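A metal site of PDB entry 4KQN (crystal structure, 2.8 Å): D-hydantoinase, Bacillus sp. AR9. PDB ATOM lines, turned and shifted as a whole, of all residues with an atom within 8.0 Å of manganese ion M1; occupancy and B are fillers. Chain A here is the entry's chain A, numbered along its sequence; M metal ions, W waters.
Manganese ion M1 is bound by OD1 of Asp 314 (2.1 Å). NE2 of His 57 binds manganese ion M1 (2.4 Å). NE2 of His 59 binds manganese ion M1, 2.5 Å away. Manganese ion M1 has three donor atoms within binding distance.
OE2 of Glu 261 sits at hydrogen-bond distance from ND1 of His 57 (3.0 Å). OG of Ser 313 lies within hydrogen-bond range of O of His 57 (3.0 Å). N of His 59 lies within hydrogen-bond range of O of His 315 (3.0 Å). A ring nitrogen (ND1) of His 59 sits at hydrogen-bond distance from the side-chain sulfur (SD) of Met 62 (3.7 Å).
Lys 149 touches manganese ion M1 (NZ to MN, 3.3 Å).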
ATOM      1  N   HIS A  57      -5.615  27.173 -19.495  1.00  0.00           N
ATOM      2  CA  HIS A  57      -5.986  26.087 -18.611  1.00  0.00           C
ATOM      3  C   HIS A  57      -7.039  25.162 -19.256  1.00  0.00           C
ATOM      4  O   HIS A  57      -8.252  25.401 -19.181  1.00  0.00           O
ATOM      5  CB  HIS A  57      -6.468  26.659 -17.287  1.00  0.00           C
ATOM      6  CG  HIS A  57      -6.465  25.687 -16.122  1.00  0.00           C
ATOM      7  ND1 HIS A  57      -6.262  26.098 -14.834  1.00  0.00           N
ATOM      8  CD2 HIS A  57      -6.690  24.354 -16.046  1.00  0.00           C
ATOM      9  CE1 HIS A  57      -6.340  25.066 -14.009  1.00  0.00           C
ATOM     10  NE2 HIS A  57      -6.609  24.003 -14.721  1.00  0.00           N
ATOM     11  N   THR A  58      -6.555  24.079 -19.855  1.00  0.00           N
ATOM     12  CA  THR A  58      -7.377  23.164 -20.608  1.00  0.00           C
ATOM     13  C   THR A  58      -6.991  21.746 -20.264  1.00  0.00           C
ATOM     14  O   THR A  58      -5.850  21.479 -19.890  1.00  0.00           O
ATOM     15  CB  THR A  58      -7.137  23.392 -22.082  1.00  0.00           C
ATOM     16  OG1 THR A  58      -5.785  23.809 -22.241  1.00  0.00           O
ATOM     17  CG2 THR A  58      -8.004  24.509 -22.592  1.00  0.00           C
ATOM     18  N   HIS A  59      -7.960  20.842 -20.342  1.00  0.00           N
ATOM     19  CA  HIS A  59      -7.679  19.424 -20.307  1.00  0.00           C
ATOM     20  C   HIS A  59      -8.556  18.792 -21.341  1.00  0.00           C
ATOM     21  O   HIS A  59      -9.651  18.280 -21.043  1.00  0.00           O
ATOM     22  CB  HIS A  59      -8.026  18.801 -18.937  1.00  0.00           C
ATOM     23  CG  HIS A  59      -7.549  19.576 -17.757  1.00  0.00           C
ATOM     24  ND1 HIS A  59      -6.344  19.318 -17.134  1.00  0.00           N
ATOM     25  CD2 HIS A  59      -8.136  20.567 -17.056  1.00  0.00           C
ATOM     26  CE1 HIS A  59      -6.214  20.138 -16.105  1.00  0.00           C
ATOM     27  NE2 HIS A  59      -7.295  20.897 -16.026  1.00  0.00           N
ATOM     28  N   MET A  62      -8.625  14.018 -21.591  1.00  0.00           N
ATOM     29  CA  MET A  62      -7.878  13.627 -20.384  1.00  0.00           C
ATOM     30  C   MET A  62      -8.553  12.436 -19.736  1.00  0.00           C
ATOM     31  O   MET A  62      -9.760  12.328 -19.771  1.00  0.00           O
ATOM     32  CB  MET A  62      -7.839  14.792 -19.380  1.00  0.00           C
ATOM     33  CG  MET A  62      -6.998  14.523 -18.117  1.00  0.00           C
ATOM     34  SD  MET A  62      -7.169  15.701 -16.756  1.00  0.00           S
ATOM     35  CE  MET A  62      -8.923  15.588 -16.472  1.00  0.00           C
ATOM     36  N   PHE A  64      -9.695  10.788 -16.263  1.00  0.00           N
ATOM     37  CA  PHE A  64      -9.999  11.223 -14.903  1.00  0.00           C
ATOM     38  C   PHE A  64     -11.278  10.463 -14.525  1.00  0.00           C
ATOM     39  O   PHE A  64     -12.270  10.534 -15.240  1.00  0.00           O
ATOM     40  CB  PHE A  64     -10.221  12.727 -14.880  1.00  0.00           C
ATOM     41  CG  PHE A  64     -10.040  13.358 -13.534  1.00  0.00           C
ATOM     42  CD1 PHE A  64     -11.107  13.418 -12.630  1.00  0.00           C
ATOM     43  CD2 PHE A  64      -8.802  13.912 -13.168  1.00  0.00           C
ATOM     44  CE1 PHE A  64     -10.940  13.987 -11.388  1.00  0.00           C
ATOM     45  CE2 PHE A  64      -8.636  14.496 -11.933  1.00  0.00           C
ATOM     46  CZ  PHE A  64      -9.701  14.530 -11.043  1.00  0.00           C
ATOM     47  N   PHE A  91      -2.714  20.611 -20.378  1.00  0.00           N
ATOM     48  CA  PHE A  91      -1.905  19.981 -19.320  1.00  0.00           C
ATOM     49  C   PHE A  91      -1.493  18.519 -19.601  1.00  0.00           C
ATOM     50  O   PHE A  91      -2.310  17.574 -19.456  1.00  0.00           O
ATOM     51  CB  PHE A  91      -2.633  20.071 -17.988  1.00  0.00           C
ATOM     52  CG  PHE A  91      -2.501  21.393 -17.339  1.00  0.00           C
ATOM     53  CD1 PHE A  91      -1.336  21.749 -16.705  1.00  0.00           C
ATOM     54  CD2 PHE A  91      -3.536  22.305 -17.395  1.00  0.00           C
ATOM     55  CE1 PHE A  91      -1.192  22.990 -16.131  1.00  0.00           C
ATOM     56  CE2 PHE A  91      -3.405  23.548 -16.831  1.00  0.00           C
ATOM     57  CZ  PHE A  91      -2.226  23.905 -16.196  1.00  0.00           C
ATOM     58  N   LYS A 149       3.254  22.090 -13.799  1.00  0.00           N
ATOM     59  CA  LYS A 149       2.200  22.007 -12.807  1.00  0.00           C
ATOM     60  C   LYS A 149       2.474  20.931 -11.790  1.00  0.00           C
ATOM     61  O   LYS A 149       2.819  19.802 -12.139  1.00  0.00           O
ATOM     62  CB  LYS A 149       0.864  21.731 -13.436  1.00  0.00           C
ATOM     63  CG  LYS A 149      -0.275  21.585 -12.428  1.00  0.00           C
ATOM     64  CD  LYS A 149      -1.595  22.079 -12.985  1.00  0.00           C
ATOM     65  CE  LYS A 149      -2.696  22.117 -11.954  1.00  0.00           C
ATOM     66  NZ  LYS A 149      -4.023  22.118 -12.605  1.00  0.00           N
ATOM     67  N   PHE A 151       0.415  19.267  -8.506  1.00  0.00           N
ATOM     68  CA  PHE A 151      -0.833  19.245  -7.776  1.00  0.00           C
ATOM     69  C   PHE A 151      -0.555  19.011  -6.310  1.00  0.00           C
ATOM     70  O   PHE A 151       0.077  18.030  -5.960  1.00  0.00           O
ATOM     71  CB  PHE A 151      -1.750  18.104  -8.228  1.00  0.00           C
ATOM     72  CG  PHE A 151      -2.388  18.304  -9.554  1.00  0.00           C
ATOM     73  CD1 PHE A 151      -1.719  17.940 -10.723  1.00  0.00           C
ATOM     74  CD2 PHE A 151      -3.689  18.807  -9.652  1.00  0.00           C
ATOM     75  CE1 PHE A 151      -2.319  18.111 -11.961  1.00  0.00           C
ATOM     76  CE2 PHE A 151      -4.268  18.984 -10.878  1.00  0.00           C
ATOM     77  CZ  PHE A 151      -3.586  18.646 -12.031  1.00  0.00           C
ATOM     78  N   TYR A 154      -5.555  15.871  -4.798  1.00  0.00           N
ATOM     79  CA  TYR A 154      -5.850  14.612  -5.464  1.00  0.00           C
ATOM     80  C   TYR A 154      -4.911  13.532  -4.985  1.00  0.00           C
ATOM     81  O   TYR A 154      -4.104  12.989  -5.750  1.00  0.00           O
ATOM     82  CB  TYR A 154      -5.783  14.748  -6.971  1.00  0.00           C
ATOM     83  CG  TYR A 154      -6.856  15.623  -7.533  1.00  0.00           C
ATOM     84  CD1 TYR A 154      -8.179  15.436  -7.201  1.00  0.00           C
ATOM     85  CD2 TYR A 154      -6.542  16.647  -8.399  1.00  0.00           C
ATOM     86  CE1 TYR A 154      -9.181  16.250  -7.728  1.00  0.00           C
ATOM     87  CE2 TYR A 154      -7.515  17.464  -8.935  1.00  0.00           C
ATOM     88  CZ  TYR A 154      -8.832  17.268  -8.594  1.00  0.00           C
ATOM     89  OH  TYR A 154      -9.799  18.090  -9.119  1.00  0.00           O
ATOM     90  N   HIS A 182      -1.809  23.623  -8.120  1.00  0.00           N
ATOM     91  CA  HIS A 182      -3.181  23.472  -7.672  1.00  0.00           C
ATOM     92  C   HIS A 182      -3.144  23.431  -6.154  1.00  0.00           C
ATOM     93  O   HIS A 182      -2.785  22.425  -5.578  1.00  0.00           O
ATOM     94  CB  HIS A 182      -3.765  22.153  -8.200  1.00  0.00           C
ATOM     95  CG  HIS A 182      -5.178  21.886  -7.754  1.00  0.00           C
ATOM     96  ND1 HIS A 182      -6.221  21.792  -8.642  1.00  0.00           N
ATOM     97  CD2 HIS A 182      -5.711  21.684  -6.524  1.00  0.00           C
ATOM     98  CE1 HIS A 182      -7.341  21.562  -7.982  1.00  0.00           C
ATOM     99  NE2 HIS A 182      -7.051  21.495  -6.690  1.00  0.00           N
ATOM    100  N   VAL A 237      -3.093  28.532  -9.992  1.00  0.00           N
ATOM    101  CA  VAL A 237      -4.227  28.402 -10.901  1.00  0.00           C
ATOM    102  C   VAL A 237      -5.573  28.198 -10.258  1.00  0.00           C
ATOM    103  O   VAL A 237      -5.710  27.521  -9.253  1.00  0.00           O
ATOM    104  CB  VAL A 237      -4.291  27.047 -11.633  1.00  0.00           C
ATOM    105  CG1 VAL A 237      -3.034  26.825 -12.444  1.00  0.00           C
ATOM    106  CG2 VAL A 237      -4.508  25.893 -10.663  1.00  0.00           C
ATOM    107  N   HIS A 238      -6.572  28.764 -10.889  1.00  0.00           N
ATOM    108  CA  HIS A 238      -7.892  28.888 -10.321  1.00  0.00           C
ATOM    109  C   HIS A 238      -8.072  29.255  -8.875  1.00  0.00           C
ATOM    110  O   HIS A 238      -8.515  28.468  -8.076  1.00  0.00           O
ATOM    111  CB  HIS A 238      -8.681  27.629 -10.604  1.00  0.00           C
ATOM    112  CG  HIS A 238      -8.004  26.367 -10.198  1.00  0.00           C
ATOM    113  ND1 HIS A 238      -7.625  26.102  -8.906  1.00  0.00           N
ATOM    114  CD2 HIS A 238      -7.740  25.239 -10.907  1.00  0.00           C
ATOM    115  CE1 HIS A 238      -7.116  24.878  -8.837  1.00  0.00           C
ATOM    116  NE2 HIS A 238      -7.179  24.341 -10.039  1.00  0.00           N
ATOM    117  N   GLU A 261      -4.522  33.280 -11.198  1.00  0.00           N
ATOM    118  CA  GLU A 261      -5.491  33.005 -12.235  1.00  0.00           C
ATOM    119  C   GLU A 261      -6.826  32.665 -11.595  1.00  0.00           C
ATOM    120  O   GLU A 261      -6.866  31.985 -10.555  1.00  0.00           O
ATOM    121  CB  GLU A 261      -4.958  31.824 -13.052  1.00  0.00           C
ATOM    122  CG  GLU A 261      -5.839  31.260 -14.185  1.00  0.00           C
ATOM    123  CD  GLU A 261      -5.473  29.786 -14.532  1.00  0.00           C
ATOM    124  OE1 GLU A 261      -4.733  29.531 -15.485  1.00  0.00           O
ATOM    125  OE2 GLU A 261      -5.945  28.875 -13.806  1.00  0.00           O
ATOM    126  N   CYS A 263     -11.117  31.567 -12.991  1.00  0.00           N
ATOM    127  CA  CYS A 263     -11.968  31.191 -14.091  1.00  0.00           C
ATOM    128  C   CYS A 263     -13.333  31.891 -13.965  1.00  0.00           C
ATOM    129  O   CYS A 263     -13.667  32.449 -12.910  1.00  0.00           O
ATOM    130  CB  CYS A 263     -12.138  29.687 -14.051  1.00  0.00           C
ATOM    131  SG  CYS A 263     -10.620  28.876 -13.499  1.00  0.00           S
ATOM    132  N   SER A 287     -12.930  21.225  -8.924  1.00  0.00           N
ATOM    133  CA  SER A 287     -12.053  21.567  -7.788  1.00  0.00           C
ATOM    134  C   SER A 287     -10.984  22.634  -8.063  1.00  0.00           C
ATOM    135  O   SER A 287     -10.142  22.450  -8.948  1.00  0.00           O
ATOM    136  CB  SER A 287     -11.372  20.286  -7.315  1.00  0.00           C
ATOM    137  OG  SER A 287     -12.339  19.335  -6.863  1.00  0.00           O
ATOM    138  N   PRO A 288     -10.961  23.735  -7.274  1.00  0.00           N
ATOM    139  CA  PRO A 288     -11.727  23.993  -6.088  1.00  0.00           C
ATOM    140  C   PRO A 288     -13.210  24.150  -6.375  1.00  0.00           C
ATOM    141  O   PRO A 288     -13.590  24.425  -7.514  1.00  0.00           O
ATOM    142  CB  PRO A 288     -11.143  25.326  -5.559  1.00  0.00           C
ATOM    143  CG  PRO A 288      -9.870  25.508  -6.290  1.00  0.00           C
ATOM    144  CD  PRO A 288     -10.131  24.893  -7.616  1.00  0.00           C
ATOM    145  N   SER A 313     -10.129  28.649 -18.339  1.00  0.00           N
ATOM    146  CA  SER A 313     -11.374  27.897 -18.221  1.00  0.00           C
ATOM    147  C   SER A 313     -11.283  26.755 -17.183  1.00  0.00           C
ATOM    148  O   SER A 313     -12.220  26.586 -16.383  1.00  0.00           O
ATOM    149  CB  SER A 313     -11.819  27.338 -19.567  1.00  0.00           C
ATOM    150  OG  SER A 313     -10.845  26.495 -20.142  1.00  0.00           O
ATOM    151  N   ASP A 314     -10.152  26.036 -17.151  1.00  0.00           N
ATOM    152  CA  ASP A 314     -10.071  24.687 -16.545  1.00  0.00           C
ATOM    153  C   ASP A 314     -11.208  23.839 -17.109  1.00  0.00           C
ATOM    154  O   ASP A 314     -11.880  23.098 -16.405  1.00  0.00           O
ATOM    155  CB  ASP A 314     -10.071  24.692 -15.011  1.00  0.00           C
ATOM    156  CG  ASP A 314      -9.651  23.335 -14.380  1.00  0.00           C
ATOM    157  OD1 ASP A 314      -8.700  22.688 -14.852  1.00  0.00           O
ATOM    158  OD2 ASP A 314     -10.246  22.931 -13.370  1.00  0.00           O
ATOM    159  N   HIS A 315     -11.428  24.011 -18.411  1.00  0.00           N
ATOM    160  CA  HIS A 315     -12.337  23.209 -19.170  1.00  0.00           C
ATOM    161  C   HIS A 315     -11.904  21.796 -19.056  1.00  0.00           C
ATOM    162  O   HIS A 315     -10.783  21.459 -19.375  1.00  0.00           O
ATOM    163  CB  HIS A 315     -12.272  23.643 -20.616  1.00  0.00           C
ATOM    164  CG  HIS A 315     -13.189  22.893 -21.509  1.00  0.00           C
ATOM    165  ND1 HIS A 315     -14.503  23.265 -21.721  1.00  0.00           N
ATOM    166  CD2 HIS A 315     -12.994  21.786 -22.268  1.00  0.00           C
ATOM    167  CE1 HIS A 315     -15.074  22.407 -22.554  1.00  0.00           C
ATOM    168  NE2 HIS A 315     -14.174  21.503 -22.910  1.00  0.00           N
ATOM    169  N   CYS A 316     -12.805  20.969 -18.559  1.00  0.00           N
ATOM    170  CA  CYS A 316     -12.542  19.562 -18.300  1.00  0.00           C
ATOM    171  C   CYS A 316     -13.903  18.873 -18.147  1.00  0.00           C
ATOM    172  O   CYS A 316     -14.388  18.692 -17.033  1.00  0.00           O
ATOM    173  CB  CYS A 316     -11.733  19.433 -17.024  1.00  0.00           C
ATOM    174  SG  CYS A 316     -11.388  17.758 -16.482  1.00  0.00           S
ATOM    175  N   ASN A 336     -14.447  15.151 -11.395  1.00  0.00           N
ATOM    176  CA  ASN A 336     -14.453  16.610 -11.156  1.00  0.00           C
ATOM    177  C   ASN A 336     -14.221  17.403 -12.411  1.00  0.00           C
ATOM    178  O   ASN A 336     -13.124  17.329 -12.930  1.00  0.00           O
ATOM    179  CB  ASN A 336     -13.281  17.001 -10.262  1.00  0.00           C
ATOM    180  CG  ASN A 336     -13.444  16.582  -8.838  1.00  0.00           C
ATOM    181  OD1 ASN A 336     -12.556  16.889  -8.043  1.00  0.00           O
ATOM    182  ND2 ASN A 336     -14.511  15.888  -8.479  1.00  0.00           N
HETATM  183 MN    MN M   1      -7.104  21.867 -13.759  1.00  0.00          MN
HETATM  184 MN    MN M   2      -6.766  22.252 -11.067  1.00  0.00          MN
HETATM  185  O   HOH W   1      -9.028  19.400 -13.794  1.00  0.00           O
